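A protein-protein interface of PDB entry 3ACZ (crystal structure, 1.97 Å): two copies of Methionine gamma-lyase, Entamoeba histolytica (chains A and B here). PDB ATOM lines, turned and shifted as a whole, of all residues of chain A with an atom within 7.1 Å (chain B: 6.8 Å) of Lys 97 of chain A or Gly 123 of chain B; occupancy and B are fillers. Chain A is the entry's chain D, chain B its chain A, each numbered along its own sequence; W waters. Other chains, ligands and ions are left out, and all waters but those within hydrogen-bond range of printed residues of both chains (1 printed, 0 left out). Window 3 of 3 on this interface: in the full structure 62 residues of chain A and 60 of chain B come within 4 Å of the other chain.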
ATOM      1  N   LEU A  95      23.908   5.176   6.503  1.00  0.00           N
ATOM      2  CA  LEU A  95      24.341   5.519   5.149  1.00  0.00           C
ATOM      3  C   LEU A  95      23.402   4.831   4.198  1.00  0.00           C
ATOM      4  O   LEU A  95      22.963   3.725   4.479  1.00  0.00           O
ATOM      5  CB  LEU A  95      25.775   5.086   4.875  1.00  0.00           C
ATOM      6  CG  LEU A  95      26.856   5.780   5.716  1.00  0.00           C
ATOM      7  CD1 LEU A  95      28.129   4.970   5.605  1.00  0.00           C
ATOM      8  CD2 LEU A  95      27.048   7.199   5.243  1.00  0.00           C
ATOM      9  N   GLN A  96      23.071   5.501   3.104  1.00  0.00           N
ATOM     10  CA  GLN A  96      22.226   4.909   2.044  1.00  0.00           C
ATOM     11  C   GLN A  96      22.744   5.253   0.638  1.00  0.00           C
ATOM     12  O   GLN A  96      23.665   6.048   0.488  1.00  0.00           O
ATOM     13  CB  GLN A  96      20.757   5.338   2.198  1.00  0.00           C
ATOM     14  CG  GLN A  96      20.497   6.836   1.994  1.00  0.00           C
ATOM     15  CD  GLN A  96      19.065   7.217   2.338  1.00  0.00           C
ATOM     16  OE1 GLN A  96      18.127   6.741   1.720  1.00  0.00           O
ATOM     17  NE2 GLN A  96      18.898   8.073   3.335  1.00  0.00           N
ATOM     18  N   LYS A  97      22.164   4.616  -0.374  1.00  0.00           N
ATOM     19  CA  LYS A  97      22.524   4.866  -1.766  1.00  0.00           C
ATOM     20  C   LYS A  97      22.625   6.381  -2.043  1.00  0.00           C
ATOM     21  O   LYS A  97      21.680   7.127  -1.788  1.00  0.00           O
ATOM     22  CB  LYS A  97      21.486   4.185  -2.675  1.00  0.00           C
ATOM     23  CG  LYS A  97      21.477   4.645  -4.139  1.00  0.00           C
ATOM     24  CD  LYS A  97      20.216   4.146  -4.846  1.00  0.00           C
ATOM     25  CE  LYS A  97      20.063   4.727  -6.263  1.00  0.00           C
ATOM     26  NZ  LYS A  97      18.897   4.066  -6.954  1.00  0.00           N
ATOM     27  N   GLY A  98      23.781   6.831  -2.535  1.00  0.00           N
ATOM     28  CA  GLY A  98      23.944   8.230  -2.906  1.00  0.00           C
ATOM     29  C   GLY A  98      24.731   9.023  -1.881  1.00  0.00           C
ATOM     30  O   GLY A  98      25.147  10.130  -2.171  1.00  0.00           O
ATOM     31  N   ASP A  99      24.913   8.460  -0.685  1.00  0.00           N
ATOM     32  CA  ASP A  99      25.707   9.083   0.378  1.00  0.00           C
ATOM     33  C   ASP A  99      27.170   8.791   0.164  1.00  0.00           C
ATOM     34  O   ASP A  99      27.526   7.827  -0.524  1.00  0.00           O
ATOM     35  CB  ASP A  99      25.326   8.545   1.761  1.00  0.00           C
ATOM     36  CG  ASP A  99      23.949   8.986   2.204  1.00  0.00           C
ATOM     37  OD1 ASP A  99      23.423   8.398   3.181  1.00  0.00           O
ATOM     38  OD2 ASP A  99      23.371   9.908   1.577  1.00  0.00           O
ATOM     39  N   HIS A 100      28.007   9.617   0.788  1.00  0.00           N
ATOM     40  CA  HIS A 100      29.443   9.505   0.691  1.00  0.00           C
ATOM     41  C   HIS A 100      30.033   9.351   2.101  1.00  0.00           C
ATOM     42  O   HIS A 100      29.625  10.052   3.023  1.00  0.00           O
ATOM     43  CB  HIS A 100      29.989  10.749  -0.062  1.00  0.00           C
ATOM     44  CG  HIS A 100      31.481  10.911  -0.008  1.00  0.00           C
ATOM     45  ND1 HIS A 100      32.354  10.019  -0.591  1.00  0.00           N
ATOM     46  CD2 HIS A 100      32.247  11.896   0.513  1.00  0.00           C
ATOM     47  CE1 HIS A 100      33.594  10.431  -0.401  1.00  0.00           C
ATOM     48  NE2 HIS A 100      33.557  11.567   0.270  1.00  0.00           N
ATOM     49  N   LEU A 119      29.873  -1.806   1.124  1.00  0.00           N
ATOM     50  CA  LEU A 119      29.245  -0.477   0.995  1.00  0.00           C
ATOM     51  C   LEU A 119      29.050  -0.012  -0.458  1.00  0.00           C
ATOM     52  O   LEU A 119      27.982   0.468  -0.788  1.00  0.00           O
ATOM     53  CB  LEU A 119      29.972   0.624   1.798  1.00  0.00           C
ATOM     54  CG  LEU A 119      30.195   0.533   3.309  1.00  0.00           C
ATOM     55  CD1 LEU A 119      30.200   1.923   3.970  1.00  0.00           C
ATOM     56  CD2 LEU A 119      29.328  -0.459   4.090  1.00  0.00           C
ATOM     57  N   ARG A 121      28.564  -1.801  -3.096  1.00  0.00           N
ATOM     58  CA  ARG A 121      27.503  -2.581  -3.687  1.00  0.00           C
ATOM     59  C   ARG A 121      26.142  -2.002  -3.281  1.00  0.00           C
ATOM     60  O   ARG A 121      25.125  -2.250  -3.924  1.00  0.00           O
ATOM     61  CB  ARG A 121      27.624  -4.050  -3.234  1.00  0.00           C
ATOM     62  CG  ARG A 121      28.861  -4.757  -3.810  1.00  0.00           C
ATOM     63  CD  ARG A 121      29.081  -6.161  -3.206  1.00  0.00           C
ATOM     64  NE  ARG A 121      27.983  -7.093  -3.423  1.00  0.00           N
ATOM     65  CZ  ARG A 121      27.840  -7.920  -4.460  1.00  0.00           C
ATOM     66  NH1 ARG A 121      26.786  -8.717  -4.507  1.00  0.00           N
ATOM     67  NH2 ARG A 121      28.717  -7.948  -5.460  1.00  0.00           N
ATOM     68  N   PHE A 122      26.116  -1.227  -2.203  1.00  0.00           N
ATOM     69  CA  PHE A 122      24.868  -0.645  -1.721  1.00  0.00           C
ATOM     70  C   PHE A 122      24.747   0.830  -2.156  1.00  0.00           C
ATOM     71  O   PHE A 122      23.913   1.582  -1.625  1.00  0.00           O
ATOM     72  CB  PHE A 122      24.766  -0.792  -0.194  1.00  0.00           C
ATOM     73  CG  PHE A 122      24.831  -2.235   0.286  1.00  0.00           C
ATOM     74  CD1 PHE A 122      25.480  -2.559   1.472  1.00  0.00           C
ATOM     75  CD2 PHE A 122      24.254  -3.266  -0.464  1.00  0.00           C
ATOM     76  CE1 PHE A 122      25.564  -3.874   1.920  1.00  0.00           C
ATOM     77  CE2 PHE A 122      24.319  -4.591  -0.020  1.00  0.00           C
ATOM     78  CZ  PHE A 122      24.987  -4.889   1.182  1.00  0.00           C
ATOM     79  N   GLY A 123      25.602   1.222  -3.105  1.00  0.00           N
ATOM     80  CA  GLY A 123      25.515   2.534  -3.759  1.00  0.00           C
ATOM     81  C   GLY A 123      26.104   3.654  -2.936  1.00  0.00           C
ATOM     82  O   GLY A 123      25.828   4.814  -3.198  1.00  0.00           O
ATOM     83  N   ILE A 124      26.920   3.298  -1.945  1.00  0.00           N
ATOM     84  CA  ILE A 124      27.554   4.241  -1.019  1.00  0.00           C
ATOM     85  C   ILE A 124      28.982   4.497  -1.487  1.00  0.00           C
ATOM     86  O   ILE A 124      29.767   3.547  -1.650  1.00  0.00           O
ATOM     87  CB  ILE A 124      27.522   3.674   0.431  1.00  0.00           C
ATOM     88  CG1 ILE A 124      26.055   3.486   0.880  1.00  0.00           C
ATOM     89  CG2 ILE A 124      28.339   4.564   1.401  1.00  0.00           C
ATOM     90  CD1 ILE A 124      25.853   2.521   2.064  1.00  0.00           C
ATOM     91  N   GLU A 125      29.299   5.769  -1.740  1.00  0.00           N
ATOM     92  CA  GLU A 125      30.645   6.182  -2.160  1.00  0.00           C
ATOM     93  C   GLU A 125      31.572   6.231  -0.960  1.00  0.00           C
ATOM     94  O   GLU A 125      31.234   6.792   0.077  1.00  0.00           O
ATOM     95  CB  GLU A 125      30.630   7.558  -2.881  1.00  0.00           C
ATOM     96  CG  GLU A 125      29.741   7.606  -4.141  1.00  0.00           C
ATOM     97  CD  GLU A 125      29.287   9.030  -4.564  1.00  0.00           C
ATOM     98  OE1 GLU A 125      28.350   9.118  -5.386  1.00  0.00           O
ATOM     99  OE2 GLU A 125      29.834  10.057  -4.090  1.00  0.00           O
ATOM    100  N   GLN B  96      22.668  -6.387  -4.919  1.00  0.00           N
ATOM    101  CA  GLN B  96      23.308  -5.099  -4.895  1.00  0.00           C
ATOM    102  C   GLN B  96      22.447  -4.038  -5.577  1.00  0.00           C
ATOM    103  O   GLN B  96      21.414  -4.348  -6.166  1.00  0.00           O
ATOM    104  CB  GLN B  96      24.711  -5.181  -5.532  1.00  0.00           C
ATOM    105  CG  GLN B  96      24.729  -5.440  -7.010  1.00  0.00           C
ATOM    106  CD  GLN B  96      26.148  -5.687  -7.506  1.00  0.00           C
ATOM    107  OE1 GLN B  96      26.917  -4.762  -7.687  1.00  0.00           O
ATOM    108  NE2 GLN B  96      26.489  -6.944  -7.718  1.00  0.00           N
ATOM    109  N   LYS B  97      22.887  -2.786  -5.490  1.00  0.00           N
ATOM    110  CA  LYS B  97      22.172  -1.685  -6.114  1.00  0.00           C
ATOM    111  C   LYS B  97      21.862  -2.002  -7.582  1.00  0.00           C
ATOM    112  O   LYS B  97      22.732  -2.448  -8.335  1.00  0.00           O
ATOM    113  CB  LYS B  97      22.981  -0.396  -6.006  1.00  0.00           C
ATOM    114  CG  LYS B  97      22.504   0.719  -6.905  1.00  0.00           C
ATOM    115  CD  LYS B  97      23.631   1.731  -7.183  1.00  0.00           C
ATOM    116  CE  LYS B  97      24.990   1.040  -7.526  1.00  0.00           C
ATOM    117  NZ  LYS B  97      26.018   2.055  -8.015  1.00  0.00           N
ATOM    118  N   GLY B  98      20.614  -1.770  -7.965  1.00  0.00           N
ATOM    119  CA  GLY B  98      20.171  -2.036  -9.339  1.00  0.00           C
ATOM    120  C   GLY B  98      19.514  -3.407  -9.506  1.00  0.00           C
ATOM    121  O   GLY B  98      18.857  -3.663 -10.524  1.00  0.00           O
ATOM    122  N   ASP B  99      19.687  -4.281  -8.510  1.00  0.00           N
ATOM    123  CA  ASP B  99      19.054  -5.618  -8.526  1.00  0.00           C
ATOM    124  C   ASP B  99      17.600  -5.542  -8.053  1.00  0.00           C
ATOM    125  O   ASP B  99      17.210  -4.602  -7.343  1.00  0.00           O
ATOM    126  CB  ASP B  99      19.793  -6.625  -7.633  1.00  0.00           C
ATOM    127  CG  ASP B  99      21.164  -7.021  -8.174  1.00  0.00           C
ATOM    128  OD1 ASP B  99      21.926  -7.632  -7.375  1.00  0.00           O
ATOM    129  OD2 ASP B  99      21.483  -6.742  -9.362  1.00  0.00           O
ATOM    130  N   HIS B 100      16.818  -6.550  -8.431  1.00  0.00           N
ATOM    131  CA  HIS B 100      15.412  -6.638  -8.047  1.00  0.00           C
ATOM    132  C   HIS B 100      15.132  -7.971  -7.307  1.00  0.00           C
ATOM    133  O   HIS B 100      15.635  -9.051  -7.667  1.00  0.00           O
ATOM    134  CB  HIS B 100      14.527  -6.404  -9.304  1.00  0.00           C
ATOM    135  CG  HIS B 100      13.069  -6.762  -9.156  1.00  0.00           C
ATOM    136  ND1 HIS B 100      12.170  -6.018  -8.399  1.00  0.00           N
ATOM    137  CD2 HIS B 100      12.334  -7.719  -9.771  1.00  0.00           C
ATOM    138  CE1 HIS B 100      10.957  -6.537  -8.521  1.00  0.00           C
ATOM    139  NE2 HIS B 100      11.032  -7.566  -9.353  1.00  0.00           N
ATOM    140  N   TRP B 118      15.178  -1.438   4.820  1.00  0.00           N
ATOM    141  CA  TRP B 118      16.623  -1.413   4.550  1.00  0.00           C
ATOM    142  C   TRP B 118      17.024  -1.681   3.091  1.00  0.00           C
ATOM    143  O   TRP B 118      17.797  -0.908   2.528  1.00  0.00           O
ATOM    144  CB  TRP B 118      17.418  -2.288   5.552  1.00  0.00           C
ATOM    145  CG  TRP B 118      17.170  -1.891   6.977  1.00  0.00           C
ATOM    146  CD1 TRP B 118      16.388  -2.561   7.893  1.00  0.00           C
ATOM    147  CD2 TRP B 118      17.653  -0.714   7.647  1.00  0.00           C
ATOM    148  NE1 TRP B 118      16.387  -1.887   9.094  1.00  0.00           N
ATOM    149  CE2 TRP B 118      17.143  -0.750   8.972  1.00  0.00           C
ATOM    150  CE3 TRP B 118      18.481   0.358   7.262  1.00  0.00           C
ATOM    151  CZ2 TRP B 118      17.424   0.251   9.915  1.00  0.00           C
ATOM    152  CZ3 TRP B 118      18.765   1.361   8.194  1.00  0.00           C
ATOM    153  CH2 TRP B 118      18.233   1.294   9.513  1.00  0.00           C
ATOM    154  N   LEU B 119      16.510  -2.734   2.466  1.00  0.00           N
ATOM    155  CA  LEU B 119      16.890  -2.997   1.060  1.00  0.00           C
ATOM    156  C   LEU B 119      16.742  -1.794   0.092  1.00  0.00           C
ATOM    157  O   LEU B 119      17.664  -1.514  -0.670  1.00  0.00           O
ATOM    158  CB  LEU B 119      16.222  -4.255   0.475  1.00  0.00           C
ATOM    159  CG  LEU B 119      16.419  -5.655   1.101  1.00  0.00           C
ATOM    160  CD1 LEU B 119      16.390  -6.791   0.066  1.00  0.00           C
ATOM    161  CD2 LEU B 119      17.552  -5.808   2.089  1.00  0.00           C
ATOM    162  N   PRO B 120      15.598  -1.074   0.123  1.00  0.00           N
ATOM    163  CA  PRO B 120      15.494   0.084  -0.774  1.00  0.00           C
ATOM    164  C   PRO B 120      16.544   1.159  -0.487  1.00  0.00           C
ATOM    165  O   PRO B 120      16.995   1.829  -1.412  1.00  0.00           O
ATOM    166  CB  PRO B 120      14.075   0.612  -0.512  1.00  0.00           C
ATOM    167  CG  PRO B 120      13.330  -0.632  -0.088  1.00  0.00           C
ATOM    168  CD  PRO B 120      14.313  -1.367   0.779  1.00  0.00           C
ATOM    169  N   ARG B 121      16.959   1.304   0.771  1.00  0.00           N
ATOM    170  CA  ARG B 121      18.001   2.283   1.102  1.00  0.00           C
ATOM    171  C   ARG B 121      19.315   1.932   0.417  1.00  0.00           C
ATOM    172  O   ARG B 121      20.141   2.793   0.196  1.00  0.00           O
ATOM    173  CB  ARG B 121      18.186   2.397   2.624  1.00  0.00           C
ATOM    174  CG  ARG B 121      17.045   3.134   3.297  1.00  0.00           C
ATOM    175  CD  ARG B 121      17.115   3.038   4.808  1.00  0.00           C
ATOM    176  NE  ARG B 121      18.259   3.752   5.359  1.00  0.00           N
ATOM    177  CZ  ARG B 121      18.258   5.043   5.676  1.00  0.00           C
ATOM    178  NH1 ARG B 121      17.169   5.791   5.479  1.00  0.00           N
ATOM    179  NH2 ARG B 121      19.358   5.600   6.163  1.00  0.00           N
ATOM    180  N   PHE B 122      19.487   0.659   0.066  1.00  0.00           N
ATOM    181  CA  PHE B 122      20.703   0.192  -0.600  1.00  0.00           C
ATOM    182  C   PHE B 122      20.522   0.046  -2.123  1.00  0.00           C
ATOM    183  O   PHE B 122      21.323  -0.616  -2.788  1.00  0.00           O
ATOM    184  CB  PHE B 122      21.190  -1.119   0.032  1.00  0.00           C
ATOM    185  CG  PHE B 122      21.394  -1.041   1.549  1.00  0.00           C
ATOM    186  CD1 PHE B 122      21.048  -2.125   2.371  1.00  0.00           C
ATOM    187  CD2 PHE B 122      21.888   0.126   2.159  1.00  0.00           C
ATOM    188  CE1 PHE B 122      21.218  -2.056   3.756  1.00  0.00           C
ATOM    189  CE2 PHE B 122      22.051   0.190   3.549  1.00  0.00           C
ATOM    190  CZ  PHE B 122      21.717  -0.913   4.339  1.00  0.00           C
ATOM    191  N   GLY B 123      19.475   0.668  -2.667  1.00  0.00           N
ATOM    192  CA  GLY B 123      19.298   0.748  -4.123  1.00  0.00           C
ATOM    193  C   GLY B 123      18.776  -0.545  -4.713  1.00  0.00           C
ATOM    194  O   GLY B 123      18.763  -0.729  -5.945  1.00  0.00           O
ATOM    195  N   ILE B 124      18.319  -1.434  -3.831  1.00  0.00           N
ATOM    196  CA  ILE B 124      17.701  -2.701  -4.248  1.00  0.00           C
ATOM    197  C   ILE B 124      16.192  -2.513  -4.370  1.00  0.00           C
ATOM    198  O   ILE B 124      15.569  -1.972  -3.465  1.00  0.00           O
ATOM    199  CB  ILE B 124      18.016  -3.828  -3.240  1.00  0.00           C
ATOM    200  CG1 ILE B 124      19.550  -3.996  -3.108  1.00  0.00           C
ATOM    201  CG2 ILE B 124      17.377  -5.190  -3.675  1.00  0.00           C
ATOM    202  CD1 ILE B 124      19.985  -4.772  -1.855  1.00  0.00           C
ATOM    203  N   GLU B 125      15.631  -2.941  -5.501  1.00  0.00           N
ATOM    204  CA  GLU B 125      14.211  -2.835  -5.805  1.00  0.00           C
ATOM    205  C   GLU B 125      13.506  -4.083  -5.269  1.00  0.00           C
ATOM    206  O   GLU B 125      13.990  -5.201  -5.444  1.00  0.00           O
ATOM    207  CB  GLU B 125      14.006  -2.737  -7.336  1.00  0.00           C
ATOM    208  CG  GLU B 125      14.760  -1.558  -7.998  1.00  0.00           C
ATOM    209  CD  GLU B 125      14.714  -1.586  -9.547  1.00  0.00           C
ATOM    210  OE1 GLU B 125      14.228  -2.554 -10.162  1.00  0.00           O
ATOM    211  OE2 GLU B 125      15.213  -0.641 -10.164  1.00  0.00           O
HETATM  212  O   HOH W   1      18.475   1.256  -7.612  1.00  0.00           O
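NH2 of Arg 121 of chain A sits close to NE2 of Gln 96 of chain B (3.3 Å). N of Lys 97 of chain B sits at hydrogen-bond distance from O of Arg 121 of chain A (2.8 Å). The backbone NH (N) of Lys 97 of chain A is in hydrogen-bond range of the backbone carbonyl oxygen (O) of Arg 121 of chain B, at 2.8 Å.
OD1 of Asp 99 of chain B sits at hydrogen-bond distance from N of Gln 96 of chain B, at 2.9 Å. The backbone NH (N) of Gly 98 of chain B is in hydrogen-bond range of the backbone carbonyl oxygen (O) of Gly 123 of chain B, 2.9 Å away. The backbone NH (N) of Gln 96 of chain A lies within hydrogen-bond range of the side-chain carboxylate (OD1) of Asp 99 of chain A (2.9 Å). O of Gly 123 of chain A lies within hydrogen-bond range of N of Gly 98 of chain A (2.9 Å).
Among the printed residues, pairs that only touch across the chains: Leu 95 of chain A with Phe 122 of chain B, Gln 96 of chain A with Arg 121 of chain B, Lys 97 of chain A with Gly 123 of chain B, Phe 122 of chain A with Phe 122 of chain B and Gly 123 of chain A with Lys 97 of chain B.
Printed residues of chain B within 4 Å of Gln 96 of chain A: Arg 121 (3.3 Å). Lys 97 of chain A touches just these residues of chain B: Arg 121 (2.8 Å) and Gly 123 (3.6 Å). His 100 of chain A touches none of the printed residues of chain B. Printed residues of chain B within 4 Å of Arg 121 of chain A: Gln 96 (3.3 Å) and Lys 97 (2.8 Å). Of the printed residues of chain A, Lys 97 of chain B touches Arg 121 and Gly 123. Gly 98 of chain B touches none of the printed residues of chain A. Of the printed residues of chain A, Arg 121 of chain B touches Gln 96 (3.3 Å) and Lys 97 (2.8 Å). Gly 123 of chain B touches just one residue of chain A: Lys 97. The nearest residue of chain A that does not touch Gly 123 of chain B is Phe 122 of chain A (4.6 Å). The nearest printed residue of chain A that does not touch Lys 97 of chain B is Phe 122 of chain A (4.4 Å).
Hydrophobic or aromatic side chains of chain B that line the printed part of chain A: Phe 122. Along chain B the printed residues that touch a printed residue of chain A span positions 96 to 123. Hydrophobic or aromatic side chains of chain A within 4 Å of the printed part of chain B: Phe 122.
Gln 96 of chain A touches Arg 121 of chain B, and with the chains exchanged Arg 121 of chain A touches Gln 96 of chain B. Lys 97 of chain A touches Arg 121 of chain B, and with the chains exchanged Arg 121 of chain A touches Lys 97 of chain B. Lys 97 of chain A touches Gly 123 of chain B, and with the chains exchanged Gly 123 of chain A touches Lys 97 of chain B. Phe 122 of chain B touches its own counterpart, Phe 122 of chain A.
Water W1 lies within hydrogen-bond range of the backbone carbonyl oxygen of Gly 123 of chain B (2.6 Å) and the side-chain amino group of Lys 97 of chain A (2.9 Å).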
